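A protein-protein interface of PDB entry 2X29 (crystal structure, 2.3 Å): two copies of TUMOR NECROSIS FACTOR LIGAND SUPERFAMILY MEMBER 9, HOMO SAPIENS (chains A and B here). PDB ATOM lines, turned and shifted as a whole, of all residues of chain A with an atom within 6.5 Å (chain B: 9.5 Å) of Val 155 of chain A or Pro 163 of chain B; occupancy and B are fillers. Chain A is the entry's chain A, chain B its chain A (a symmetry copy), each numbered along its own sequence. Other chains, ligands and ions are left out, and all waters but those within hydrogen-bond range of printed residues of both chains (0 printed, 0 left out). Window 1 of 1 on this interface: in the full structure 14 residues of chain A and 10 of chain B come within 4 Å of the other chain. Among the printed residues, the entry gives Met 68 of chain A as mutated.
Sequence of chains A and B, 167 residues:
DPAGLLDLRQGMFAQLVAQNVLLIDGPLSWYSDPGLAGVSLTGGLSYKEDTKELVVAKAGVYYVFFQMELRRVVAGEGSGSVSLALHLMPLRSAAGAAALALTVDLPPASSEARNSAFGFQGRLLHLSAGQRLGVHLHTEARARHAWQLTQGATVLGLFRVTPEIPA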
ATOM      1  N   PHE A  13      -1.236 -16.802   5.232  1.00  0.00           N
ATOM      2  CA  PHE A  13      -1.177 -16.091   6.500  1.00  0.00           C
ATOM      3  C   PHE A  13       0.282 -16.023   6.919  1.00  0.00           C
ATOM      4  O   PHE A  13       1.016 -17.004   6.713  1.00  0.00           O
ATOM      5  CB  PHE A  13      -1.944 -16.916   7.565  1.00  0.00           C
ATOM      6  CG  PHE A  13      -1.770 -16.408   8.983  1.00  0.00           C
ATOM      7  CD1 PHE A  13      -2.312 -15.148   9.385  1.00  0.00           C
ATOM      8  CD2 PHE A  13      -1.116 -17.199   9.927  1.00  0.00           C
ATOM      9  CE1 PHE A  13      -2.190 -14.692  10.686  1.00  0.00           C
ATOM     10  CE2 PHE A  13      -0.978 -16.768  11.189  1.00  0.00           C
ATOM     11  CZ  PHE A  13      -1.496 -15.491  11.592  1.00  0.00           C
ATOM     12  N   GLN A  15       2.804 -14.469  10.420  1.00  0.00           N
ATOM     13  CA  GLN A  15       2.850 -13.811  11.725  1.00  0.00           C
ATOM     14  C   GLN A  15       4.253 -13.626  12.142  1.00  0.00           C
ATOM     15  O   GLN A  15       5.106 -14.438  11.811  1.00  0.00           O
ATOM     16  CB  GLN A  15       2.074 -14.587  12.813  1.00  0.00           C
ATOM     17  CG  GLN A  15       2.538 -16.027  13.036  1.00  0.00           C
ATOM     18  CD  GLN A  15       1.425 -16.775  13.828  1.00  0.00           C
ATOM     19  OE1 GLN A  15       0.656 -16.128  14.530  1.00  0.00           O
ATOM     20  NE2 GLN A  15       1.371 -18.110  13.725  1.00  0.00           N
ATOM     21  N   LEU A  16       4.481 -12.515  12.863  1.00  0.00           N
ATOM     22  CA  LEU A  16       5.770 -12.151  13.317  1.00  0.00           C
ATOM     23  C   LEU A  16       5.754 -11.979  14.832  1.00  0.00           C
ATOM     24  O   LEU A  16       4.799 -11.455  15.397  1.00  0.00           O
ATOM     25  CB  LEU A  16       6.271 -10.845  12.631  1.00  0.00           C
ATOM     26  CG  LEU A  16       6.474 -10.938  11.107  1.00  0.00           C
ATOM     27  CD1 LEU A  16       6.653  -9.550  10.537  1.00  0.00           C
ATOM     28  CD2 LEU A  16       7.630 -11.844  10.723  1.00  0.00           C
ATOM     29  N   VAL A  17       6.829 -12.452  15.490  1.00  0.00           N
ATOM     30  CA  VAL A  17       6.946 -12.364  16.977  1.00  0.00           C
ATOM     31  C   VAL A  17       7.907 -11.226  17.296  1.00  0.00           C
ATOM     32  O   VAL A  17       8.939 -11.098  16.617  1.00  0.00           O
ATOM     33  CB  VAL A  17       7.554 -13.646  17.551  1.00  0.00           C
ATOM     34  CG1 VAL A  17       7.661 -13.593  19.065  1.00  0.00           C
ATOM     35  CG2 VAL A  17       6.669 -14.868  17.107  1.00  0.00           C
ATOM     36  N   ALA A  18       7.583 -10.406  18.298  1.00  0.00           N
ATOM     37  CA  ALA A  18       8.485  -9.316  18.728  1.00  0.00           C
ATOM     38  C   ALA A  18       9.601  -9.917  19.610  1.00  0.00           C
ATOM     39  O   ALA A  18       9.351 -10.703  20.536  1.00  0.00           O
ATOM     40  CB  ALA A  18       7.702  -8.244  19.534  1.00  0.00           C
ATOM     41  N   TRP A  30      11.034  -7.563  14.907  1.00  0.00           N
ATOM     42  CA  TRP A  30      10.226  -8.713  14.599  1.00  0.00           C
ATOM     43  C   TRP A  30      11.074  -9.793  13.995  1.00  0.00           C
ATOM     44  O   TRP A  30      12.045  -9.510  13.254  1.00  0.00           O
ATOM     45  CB  TRP A  30       9.112  -8.348  13.598  1.00  0.00           C
ATOM     46  CG  TRP A  30       8.253  -7.287  14.100  1.00  0.00           C
ATOM     47  CD1 TRP A  30       8.346  -5.932  13.789  1.00  0.00           C
ATOM     48  CD2 TRP A  30       7.120  -7.422  15.014  1.00  0.00           C
ATOM     49  NE1 TRP A  30       7.358  -5.225  14.481  1.00  0.00           N
ATOM     50  CE2 TRP A  30       6.583  -6.099  15.210  1.00  0.00           C
ATOM     51  CE3 TRP A  30       6.481  -8.517  15.625  1.00  0.00           C
ATOM     52  CZ2 TRP A  30       5.475  -5.839  16.056  1.00  0.00           C
ATOM     53  CZ3 TRP A  30       5.382  -8.248  16.461  1.00  0.00           C
ATOM     54  CH2 TRP A  30       4.865  -6.933  16.612  1.00  0.00           C
ATOM     55  N   LEU A  36       5.952 -21.640  14.428  1.00  0.00           N
ATOM     56  CA  LEU A  36       4.568 -21.107  14.361  1.00  0.00           C
ATOM     57  C   LEU A  36       4.106 -21.288  12.950  1.00  0.00           C
ATOM     58  O   LEU A  36       4.930 -21.301  12.005  1.00  0.00           O
ATOM     59  CB  LEU A  36       4.480 -19.615  14.793  1.00  0.00           C
ATOM     60  CG  LEU A  36       4.976 -19.342  16.249  1.00  0.00           C
ATOM     61  CD1 LEU A  36       4.666 -17.916  16.693  1.00  0.00           C
ATOM     62  CD2 LEU A  36       4.392 -20.349  17.212  1.00  0.00           C
ATOM     63  N   ALA A  37       2.791 -21.441  12.806  1.00  0.00           N
ATOM     64  CA  ALA A  37       2.133 -21.497  11.486  1.00  0.00           C
ATOM     65  C   ALA A  37       2.422 -20.226  10.688  1.00  0.00           C
ATOM     66  O   ALA A  37       2.705 -19.172  11.248  1.00  0.00           O
ATOM     67  CB  ALA A  37       0.618 -21.676  11.643  1.00  0.00           C
ATOM     68  N   PHE A  65      -3.488  -7.950  12.504  1.00  0.00           N
ATOM     69  CA  PHE A  65      -3.779  -7.826  13.932  1.00  0.00           C
ATOM     70  C   PHE A  65      -2.514  -7.696  14.786  1.00  0.00           C
ATOM     71  O   PHE A  65      -1.421  -8.110  14.376  1.00  0.00           O
ATOM     72  CB  PHE A  65      -4.711  -8.967  14.431  1.00  0.00           C
ATOM     73  CG  PHE A  65      -4.069 -10.366  14.440  1.00  0.00           C
ATOM     74  CD1 PHE A  65      -3.162 -10.720  15.420  1.00  0.00           C
ATOM     75  CD2 PHE A  65      -4.372 -11.296  13.440  1.00  0.00           C
ATOM     76  CE1 PHE A  65      -2.573 -11.953  15.446  1.00  0.00           C
ATOM     77  CE2 PHE A  65      -3.803 -12.557  13.462  1.00  0.00           C
ATOM     78  CZ  PHE A  65      -2.920 -12.903  14.490  1.00  0.00           C
ATOM     79  N   PHE A  66      -2.695  -7.132  15.973  1.00  0.00           N
ATOM     80  CA  PHE A  66      -1.673  -7.073  16.951  1.00  0.00           C
ATOM     81  C   PHE A  66      -2.183  -7.879  18.137  1.00  0.00           C
ATOM     82  O   PHE A  66      -3.288  -7.700  18.576  1.00  0.00           O
ATOM     83  CB  PHE A  66      -1.586  -5.689  17.577  1.00  0.00           C
ATOM     84  CG  PHE A  66      -0.884  -4.698  16.801  1.00  0.00           C
ATOM     85  CD1 PHE A  66      -1.310  -3.350  16.857  1.00  0.00           C
ATOM     86  CD2 PHE A  66       0.221  -5.025  16.103  1.00  0.00           C
ATOM     87  CE1 PHE A  66      -0.641  -2.404  16.197  1.00  0.00           C
ATOM     88  CE2 PHE A  66       0.897  -4.047  15.414  1.00  0.00           C
ATOM     89  CZ  PHE A  66       0.437  -2.740  15.446  1.00  0.00           C
ATOM     90  N   GLN A  67      -1.290  -8.627  18.751  1.00  0.00           N
ATOM     91  CA  GLN A  67      -1.587  -9.161  20.051  1.00  0.00           C
ATOM     92  C   GLN A  67      -0.532  -8.706  21.018  1.00  0.00           C
ATOM     93  O   GLN A  67       0.664  -8.748  20.728  1.00  0.00           O
ATOM     94  CB  GLN A  67      -1.667 -10.723  20.026  1.00  0.00           C
ATOM     95  CG  GLN A  67      -1.501 -11.316  21.381  1.00  0.00           C
ATOM     96  CD  GLN A  67      -1.514 -12.868  21.411  1.00  0.00           C
ATOM     97  OE1 GLN A  67      -0.477 -13.517  21.411  1.00  0.00           O
ATOM     98  NE2 GLN A  67      -2.673 -13.435  21.462  1.00  0.00           N
ATOM     99  N   MET A  68      -0.912  -8.316  22.215  1.00  0.00           N
ATOM    100  CA  MET A  68       0.165  -8.029  23.186  1.00  0.00           C
ATOM    101  C   MET A  68      -0.105  -8.536  24.594  1.00  0.00           C
ATOM    102  O   MET A  68      -1.166  -8.336  25.156  1.00  0.00           O
ATOM    103  CB  MET A  68       0.467  -6.519  23.198  1.00  0.00           C
ATOM    104  CG  MET A  68       1.408  -6.155  24.204  1.00  0.00           C
ATOM    105  SD  MET A  68       1.885  -4.216  24.085  1.00  0.00           S
ATOM    106  CE  MET A  68       0.084  -3.397  24.042  1.00  0.00           C
ATOM    107  N   LEU A  84       0.591   0.166  20.999  1.00  0.00           N
ATOM    108  CA  LEU A  84       1.267  -0.239  19.741  1.00  0.00           C
ATOM    109  C   LEU A  84       0.612   0.482  18.599  1.00  0.00           C
ATOM    110  O   LEU A  84      -0.626   0.701  18.645  1.00  0.00           O
ATOM    111  CB  LEU A  84       1.110  -1.727  19.490  1.00  0.00           C
ATOM    112  CG  LEU A  84       1.747  -2.654  20.454  1.00  0.00           C
ATOM    113  CD1 LEU A  84       1.529  -4.083  19.924  1.00  0.00           C
ATOM    114  CD2 LEU A  84       3.240  -2.328  20.612  1.00  0.00           C
ATOM    115  N   GLY A 152       7.814 -13.678  23.603  1.00  0.00           N
ATOM    116  CA  GLY A 152       7.208 -14.477  22.561  1.00  0.00           C
ATOM    117  C   GLY A 152       5.673 -14.299  22.382  1.00  0.00           C
ATOM    118  O   GLY A 152       5.083 -14.971  21.512  1.00  0.00           O
ATOM    119  N   ALA A 153       5.027 -13.386  23.131  1.00  0.00           N
ATOM    120  CA  ALA A 153       3.557 -13.265  23.043  1.00  0.00           C
ATOM    121  C   ALA A 153       3.130 -11.937  22.394  1.00  0.00           C
ATOM    122  O   ALA A 153       1.949 -11.581  22.385  1.00  0.00           O
ATOM    123  CB  ALA A 153       2.914 -13.448  24.432  1.00  0.00           C
ATOM    124  N   THR A 154       4.085 -11.176  21.843  1.00  0.00           N
ATOM    125  CA  THR A 154       3.704 -10.022  21.096  1.00  0.00           C
ATOM    126  C   THR A 154       3.818 -10.380  19.622  1.00  0.00           C
ATOM    127  O   THR A 154       4.907 -10.678  19.156  1.00  0.00           O
ATOM    128  CB  THR A 154       4.500  -8.784  21.478  1.00  0.00           C
ATOM    129  OG1 THR A 154       4.128  -8.440  22.817  1.00  0.00           O
ATOM    130  CG2 THR A 154       4.142  -7.553  20.580  1.00  0.00           C
ATOM    131  N   VAL A 155       2.685 -10.311  18.906  1.00  0.00           N
ATOM    132  CA  VAL A 155       2.573 -10.887  17.582  1.00  0.00           C
ATOM    133  C   VAL A 155       1.908  -9.889  16.672  1.00  0.00           C
ATOM    134  O   VAL A 155       0.982  -9.239  17.097  1.00  0.00           O
ATOM    135  CB  VAL A 155       1.743 -12.210  17.576  1.00  0.00           C
ATOM    136  CG1 VAL A 155       1.631 -12.753  16.155  1.00  0.00           C
ATOM    137  CG2 VAL A 155       2.389 -13.233  18.621  1.00  0.00           C
ATOM    138  N   LEU A 156       2.398  -9.802  15.427  1.00  0.00           N
ATOM    139  CA  LEU A 156       1.762  -9.106  14.352  1.00  0.00           C
ATOM    140  C   LEU A 156       1.320 -10.134  13.270  1.00  0.00           C
ATOM    141  O   LEU A 156       2.147 -10.894  12.727  1.00  0.00           O
ATOM    142  CB  LEU A 156       2.740  -8.119  13.751  1.00  0.00           C
ATOM    143  CG  LEU A 156       2.286  -7.476  12.406  1.00  0.00           C
ATOM    144  CD1 LEU A 156       1.076  -6.584  12.623  1.00  0.00           C
ATOM    145  CD2 LEU A 156       3.478  -6.711  11.657  1.00  0.00           C
ATOM    146  N   GLY A 157       0.014 -10.224  13.020  1.00  0.00           N
ATOM    147  CA  GLY A 157      -0.519 -11.185  12.083  1.00  0.00           C
ATOM    148  C   GLY A 157      -1.032 -10.492  10.815  1.00  0.00           C
ATOM    149  O   GLY A 157      -1.710  -9.415  10.904  1.00  0.00           O
ATOM    150  N   LEU B   8      -7.923 -26.545  20.679  1.00  0.00           N
ATOM    151  CA  LEU B   8      -7.738 -26.084  19.291  1.00  0.00           C
ATOM    152  C   LEU B   8      -6.350 -25.511  19.089  1.00  0.00           C
ATOM    153  O   LEU B   8      -5.903 -24.680  19.894  1.00  0.00           O
ATOM    154  CB  LEU B   8      -8.771 -25.002  18.905  1.00  0.00           C
ATOM    155  CG  LEU B   8     -10.241 -25.362  18.866  1.00  0.00           C
ATOM    156  CD1 LEU B   8     -10.994 -24.132  18.374  1.00  0.00           C
ATOM    157  CD2 LEU B   8     -10.467 -26.483  17.856  1.00  0.00           C
ATOM    158  N   ARG B   9      -5.702 -25.939  18.011  1.00  0.00           N
ATOM    159  CA  ARG B   9      -4.467 -25.291  17.527  1.00  0.00           C
ATOM    160  C   ARG B   9      -4.858 -24.013  16.830  1.00  0.00           C
ATOM    161  O   ARG B   9      -6.004 -23.847  16.445  1.00  0.00           O
ATOM    162  CB  ARG B   9      -3.587 -26.208  16.569  1.00  0.00           C
ATOM    163  CG  ARG B   9      -2.846 -27.392  17.437  1.00  0.00           C
ATOM    164  CD  ARG B   9      -2.012 -28.462  16.629  1.00  0.00           C
ATOM    165  NE  ARG B   9      -2.733 -29.032  15.458  1.00  0.00           N
ATOM    166  CZ  ARG B   9      -3.222 -30.295  15.368  1.00  0.00           C
ATOM    167  NH1 ARG B   9      -3.081 -31.173  16.383  1.00  0.00           N
ATOM    168  NH2 ARG B   9      -3.852 -30.709  14.258  1.00  0.00           N
ATOM    169  N   GLN B  10      -3.930 -23.095  16.710  1.00  0.00           N
ATOM    170  CA  GLN B  10      -4.118 -21.956  15.869  1.00  0.00           C
ATOM    171  C   GLN B  10      -4.685 -22.297  14.467  1.00  0.00           C
ATOM    172  O   GLN B  10      -4.141 -23.147  13.779  1.00  0.00           O
ATOM    173  CB  GLN B  10      -2.803 -21.172  15.719  1.00  0.00           C
ATOM    174  CG  GLN B  10      -3.000 -19.860  14.844  1.00  0.00           C
ATOM    175  CD  GLN B  10      -1.704 -19.013  14.812  1.00  0.00           C
ATOM    176  OE1 GLN B  10      -0.625 -19.556  14.780  1.00  0.00           O
ATOM    177  NE2 GLN B  10      -1.836 -17.686  14.846  1.00  0.00           N
ATOM    178  N   GLY B  11      -5.723 -21.594  14.038  1.00  0.00           N
ATOM    179  CA  GLY B  11      -6.164 -21.739  12.637  1.00  0.00           C
ATOM    180  C   GLY B  11      -7.150 -22.924  12.513  1.00  0.00           C
ATOM    181  O   GLY B  11      -7.667 -23.200  11.424  1.00  0.00           O
ATOM    182  N   LYS B  58      -6.650 -24.081  25.428  1.00  0.00           N
ATOM    183  CA  LYS B  58      -5.586 -23.123  25.129  1.00  0.00           C
ATOM    184  C   LYS B  58      -6.005 -21.638  25.217  1.00  0.00           C
ATOM    185  O   LYS B  58      -7.032 -21.197  24.685  1.00  0.00           O
ATOM    186  CB  LYS B  58      -4.992 -23.432  23.770  1.00  0.00           C
ATOM    187  CG  LYS B  58      -4.356 -24.833  23.599  1.00  0.00           C
ATOM    188  CD  LYS B  58      -3.244 -24.949  24.637  1.00  0.00           C
ATOM    189  CE  LYS B  58      -2.647 -26.331  24.760  1.00  0.00           C
ATOM    190  NZ  LYS B  58      -2.421 -26.770  23.390  1.00  0.00           N
ATOM    191  N   ALA B  59      -5.215 -20.875  25.925  1.00  0.00           N
ATOM    192  CA  ALA B  59      -5.367 -19.409  26.007  1.00  0.00           C
ATOM    193  C   ALA B  59      -5.260 -18.801  24.612  1.00  0.00           C
ATOM    194  O   ALA B  59      -4.359 -19.127  23.862  1.00  0.00           O
ATOM    195  CB  ALA B  59      -4.247 -18.812  26.897  1.00  0.00           C
ATOM    196  N   GLY B  60      -6.110 -17.860  24.270  1.00  0.00           N
ATOM    197  CA  GLY B  60      -5.971 -17.272  22.949  1.00  0.00           C
ATOM    198  C   GLY B  60      -7.138 -16.399  22.707  1.00  0.00           C
ATOM    199  O   GLY B  60      -8.081 -16.327  23.529  1.00  0.00           O
ATOM    200  N   VAL B  61      -7.087 -15.731  21.551  1.00  0.00           N
ATOM    201  CA  VAL B  61      -8.227 -15.036  21.046  1.00  0.00           C
ATOM    202  C   VAL B  61      -8.938 -15.981  19.996  1.00  0.00           C
ATOM    203  O   VAL B  61      -8.271 -16.478  19.042  1.00  0.00           O
ATOM    204  CB  VAL B  61      -7.809 -13.690  20.357  1.00  0.00           C
ATOM    205  CG1 VAL B  61      -9.081 -13.017  19.722  1.00  0.00           C
ATOM    206  CG2 VAL B  61      -7.172 -12.713  21.383  1.00  0.00           C
ATOM    207  N   TYR B  62     -10.252 -16.115  20.138  1.00  0.00           N
ATOM    208  CA  TYR B  62     -11.062 -16.974  19.290  1.00  0.00           C
ATOM    209  C   TYR B  62     -12.152 -16.125  18.667  1.00  0.00           C
ATOM    210  O   TYR B  62     -12.729 -15.268  19.345  1.00  0.00           O
ATOM    211  CB  TYR B  62     -11.741 -18.110  20.118  1.00  0.00           C
ATOM    212  CG  TYR B  62     -10.755 -19.099  20.752  1.00  0.00           C
ATOM    213  CD1 TYR B  62      -9.973 -18.747  21.904  1.00  0.00           C
ATOM    214  CD2 TYR B  62     -10.588 -20.391  20.198  1.00  0.00           C
ATOM    215  CE1 TYR B  62      -9.037 -19.716  22.505  1.00  0.00           C
ATOM    216  CE2 TYR B  62      -9.715 -21.339  20.771  1.00  0.00           C
ATOM    217  CZ  TYR B  62      -8.949 -21.000  21.908  1.00  0.00           C
ATOM    218  OH  TYR B  62      -8.074 -21.957  22.344  1.00  0.00           O
ATOM    219  N   HIS B 126     -11.193 -13.077  24.024  1.00  0.00           N
ATOM    220  CA  HIS B 126     -10.003 -13.581  24.671  1.00  0.00           C
ATOM    221  C   HIS B 126     -10.431 -14.668  25.661  1.00  0.00           C
ATOM    222  O   HIS B 126     -11.204 -14.410  26.523  1.00  0.00           O
ATOM    223  CB  HIS B 126      -9.257 -12.436  25.404  1.00  0.00           C
ATOM    224  CG  HIS B 126      -8.103 -12.931  26.215  1.00  0.00           C
ATOM    225  ND1 HIS B 126      -7.257 -13.918  25.761  1.00  0.00           N
ATOM    226  CD2 HIS B 126      -7.638 -12.576  27.437  1.00  0.00           C
ATOM    227  CE1 HIS B 126      -6.317 -14.154  26.663  1.00  0.00           C
ATOM    228  NE2 HIS B 126      -6.528 -13.354  27.693  1.00  0.00           N
ATOM    229  N   LEU B 127      -9.917 -15.880  25.502  1.00  0.00           N
ATOM    230  CA  LEU B 127     -10.185 -16.978  26.450  1.00  0.00           C
ATOM    231  C   LEU B 127      -8.895 -17.543  27.042  1.00  0.00           C
ATOM    232  O   LEU B 127      -8.043 -18.097  26.308  1.00  0.00           O
ATOM    233  CB  LEU B 127     -10.975 -18.098  25.770  1.00  0.00           C
ATOM    234  CG  LEU B 127     -12.217 -17.577  25.014  1.00  0.00           C
ATOM    235  CD1 LEU B 127     -12.798 -18.675  24.060  1.00  0.00           C
ATOM    236  CD2 LEU B 127     -13.369 -17.028  25.999  1.00  0.00           C
ATOM    237  N   ARG B 160      -9.762 -20.537  16.396  1.00  0.00           N
ATOM    238  CA  ARG B 160      -8.603 -19.972  17.077  1.00  0.00           C
ATOM    239  C   ARG B 160      -7.729 -19.075  16.175  1.00  0.00           C
ATOM    240  O   ARG B 160      -7.157 -19.557  15.190  1.00  0.00           O
ATOM    241  CB  ARG B 160      -7.716 -21.065  17.638  1.00  0.00           C
ATOM    242  CG  ARG B 160      -6.657 -20.485  18.605  1.00  0.00           C
ATOM    243  CD  ARG B 160      -5.908 -21.505  19.452  1.00  0.00           C
ATOM    244  NE  ARG B 160      -4.618 -20.930  19.873  1.00  0.00           N
ATOM    245  CZ  ARG B 160      -3.599 -21.651  20.343  1.00  0.00           C
ATOM    246  NH1 ARG B 160      -3.741 -22.966  20.521  1.00  0.00           N
ATOM    247  NH2 ARG B 160      -2.460 -21.029  20.695  1.00  0.00           N
ATOM    248  N   VAL B 161      -7.610 -17.802  16.525  1.00  0.00           N
ATOM    249  CA  VAL B 161      -6.861 -16.800  15.687  1.00  0.00           C
ATOM    250  C   VAL B 161      -5.379 -16.751  16.042  1.00  0.00           C
ATOM    251  O   VAL B 161      -4.513 -16.554  15.153  1.00  0.00           O
ATOM    252  CB  VAL B 161      -7.481 -15.347  15.872  1.00  0.00           C
ATOM    253  CG1 VAL B 161      -6.653 -14.330  15.204  1.00  0.00           C
ATOM    254  CG2 VAL B 161      -8.983 -15.310  15.370  1.00  0.00           C
ATOM    255  N   THR B 162      -5.072 -16.920  17.344  1.00  0.00           N
ATOM    256  CA  THR B 162      -3.737 -16.557  17.844  1.00  0.00           C
ATOM    257  C   THR B 162      -2.852 -17.775  18.126  1.00  0.00           C
ATOM    258  O   THR B 162      -3.380 -18.905  18.337  1.00  0.00           O
ATOM    259  CB  THR B 162      -3.855 -15.739  19.163  1.00  0.00           C
ATOM    260  OG1 THR B 162      -4.693 -16.415  20.096  1.00  0.00           O
ATOM    261  CG2 THR B 162      -4.407 -14.376  18.915  1.00  0.00           C
ATOM    262  N   PRO B 163      -1.513 -17.568  18.168  1.00  0.00           N
ATOM    263  CA  PRO B 163      -0.580 -18.720  18.345  1.00  0.00           C
ATOM    264  C   PRO B 163      -0.154 -18.958  19.766  1.00  0.00           C
ATOM    265  O   PRO B 163      -0.467 -18.169  20.673  1.00  0.00           O
ATOM    266  CB  PRO B 163       0.680 -18.298  17.532  1.00  0.00           C
ATOM    267  CG  PRO B 163       0.676 -16.676  17.932  1.00  0.00           C
ATOM    268  CD  PRO B 163      -0.806 -16.340  17.746  1.00  0.00           C
ATOM    269  N   GLU B 164       0.525 -20.079  19.959  1.00  0.00           N
ATOM    270  CA  GLU B 164       1.335 -20.311  21.160  1.00  0.00           C
ATOM    271  C   GLU B 164       2.556 -19.402  21.142  1.00  0.00           C
ATOM    272  O   GLU B 164       2.990 -18.924  20.080  1.00  0.00           O
ATOM    273  CB  GLU B 164       1.885 -21.751  21.165  1.00  0.00           C
ATOM    274  CG  GLU B 164       0.819 -22.806  21.221  1.00  0.00           C
ATOM    275  CD  GLU B 164       0.101 -22.771  22.585  1.00  0.00           C
ATOM    276  OE1 GLU B 164      -1.087 -22.323  22.656  1.00  0.00           O
ATOM    277  OE2 GLU B 164       0.736 -23.214  23.573  1.00  0.00           O
ATOM    278  N   ILE B 165       3.150 -19.263  22.322  1.00  0.00           N
ATOM    279  CA  ILE B 165       4.517 -18.767  22.546  1.00  0.00           C
ATOM    280  C   ILE B 165       5.504 -19.734  21.916  1.00  0.00           C
ATOM    281  O   ILE B 165       5.406 -20.915  22.169  1.00  0.00           O
ATOM    282  CB  ILE B 165       4.751 -18.670  24.089  1.00  0.00           C
ATOM    283  CG1 ILE B 165       3.706 -17.647  24.653  1.00  0.00           C
ATOM    284  CG2 ILE B 165       6.260 -18.334  24.428  1.00  0.00           C
ATOM    285  CD1 ILE B 165       3.519 -17.671  26.104  1.00  0.00           C
ATOM    286  N   PRO B 166       6.437 -19.237  21.060  1.00  0.00           N
ATOM    287  CA  PRO B 166       7.497 -20.090  20.434  1.00  0.00           C
ATOM    288  C   PRO B 166       8.280 -20.897  21.525  1.00  0.00           C
ATOM    289  O   PRO B 166       8.573 -20.343  22.619  1.00  0.00           O
ATOM    290  CB  PRO B 166       8.443 -19.067  19.815  1.00  0.00           C
ATOM    291  CG  PRO B 166       7.587 -17.768  19.674  1.00  0.00           C
ATOM    292  CD  PRO B 166       6.577 -17.796  20.740  1.00  0.00           C
ATOM    293  N   ALA B 167       8.593 -22.167  21.230  1.00  0.00           N
ATOM    294  CA  ALA B 167       9.377 -23.109  22.111  1.00  0.00           C
ATOM    295  C   ALA B 167      10.816 -22.586  22.360  1.00  0.00           C
ATOM    296  O   ALA B 167      11.318 -21.808  21.513  1.00  0.00           O
ATOM    297  CB  ALA B 167       9.410 -24.525  21.468  1.00  0.00           C
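The side-chain amide nitrogen of Gln 15 of chain A sits at hydrogen-bond distance from the side-chain amide oxygen of Gln 10 of chain B (2.7 Å).
The guanidinium group of Arg 160 of chain B sits close to the backbone carbonyl oxygen of Pro 163 of chain B (3.5 Å).
The side-chain hydroxyl (OG1) of Thr 162 of chain B is in hydrogen-bond range of the backbone NH (N) of Val 61 of chain B, at 2.9 Å.
NE2 of Gln 10 of chain B is in hydrogen-bond range of O of Val 161 of chain B, at 2.9 Å.
The guanidinium group (NE) of Arg 160 of chain B sits at hydrogen-bond distance from the backbone carbonyl oxygen (O) of Thr 162 of chain B (2.8 Å).
The backbone carbonyl oxygen of Val 61 of chain B is in hydrogen-bond range of the backbone NH of Val 161 of chain B.
OE1 of Gln 67 of chain A sits close to O of Ala 153 of chain A, at 3.3 Å.
NE2 of Gln 10 of chain B touches CE2 of Phe 13 of chain A, 3.9 Å away.
CG of Pro 163 of chain B touches OE1 of Gln 15 of chain A, at 3.4 Å.
Val 17 of chain A touches Pro 166 of chain B.
Glu 164 of chain B touches Leu 36 of chain A (O to CD2, 3.5 Å).
Gln 10 of chain B touches Ala 37 of chain A.
Val 161 of chain B touches Phe 65 of chain A.
Thr 162 of chain B touches Gln 67 of chain A (CG2 to NE2, 3.2 Å).
Ile 165 of chain B touches Gly 152 of chain A.
Gly 152 of chain A touches Pro 166 of chain B.
Val 155 of chain A touches Pro 163 of chain B (CG2 to CG, 3.9 Å).
No position is printed for both chains.
Of the 11 pairs that touch across the chains among the printed residues, none has its exchanged pair printed and touching as well.
Printed residues of chain B within 4 Å of Phe 65 of chain A: Val 161 (3.8 Å).
Of the printed residues of chain B, Gln 67 of chain A touches Thr 162 (3.2 Å).
Val 155 of chain A touches just one residue of chain B: Pro 163.
Of the printed residues of chain A, Gln 10 of chain B touches Phe 13 (3.9 Å), Gln 15 (2.7 Å) and Ala 37 (3.98 Å).
Of chain A, only Gln 15 (3.4 Å) and Val 155 (3.9 Å) come within 4 Å of Pro 163 of chain B.
Printed residues of chain A within 4 Å of Ile 165 of chain B: Gly 152 (3.97 Å).
Of the printed residues of chain A, Pro 166 of chain B touches Val 17 (3.98 Å) and Gly 152 (3.3 Å).
Of the 19 printed residues of chain A, 9 touch a printed residue of chain B.
Of the 19 printed residues of chain B, 7 touch a printed residue of chain A.
Hydrophobic or aromatic side chains of chain B that line the printed part of chain A: Val 161, Pro 163 and Pro 166.
Among the printed residues, 11 pairs touch across the chains.
Among the printed residues, no Asp or Glu carboxylate lies within 4 Å of a Lys or Arg side-chain nitrogen of the other chain.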
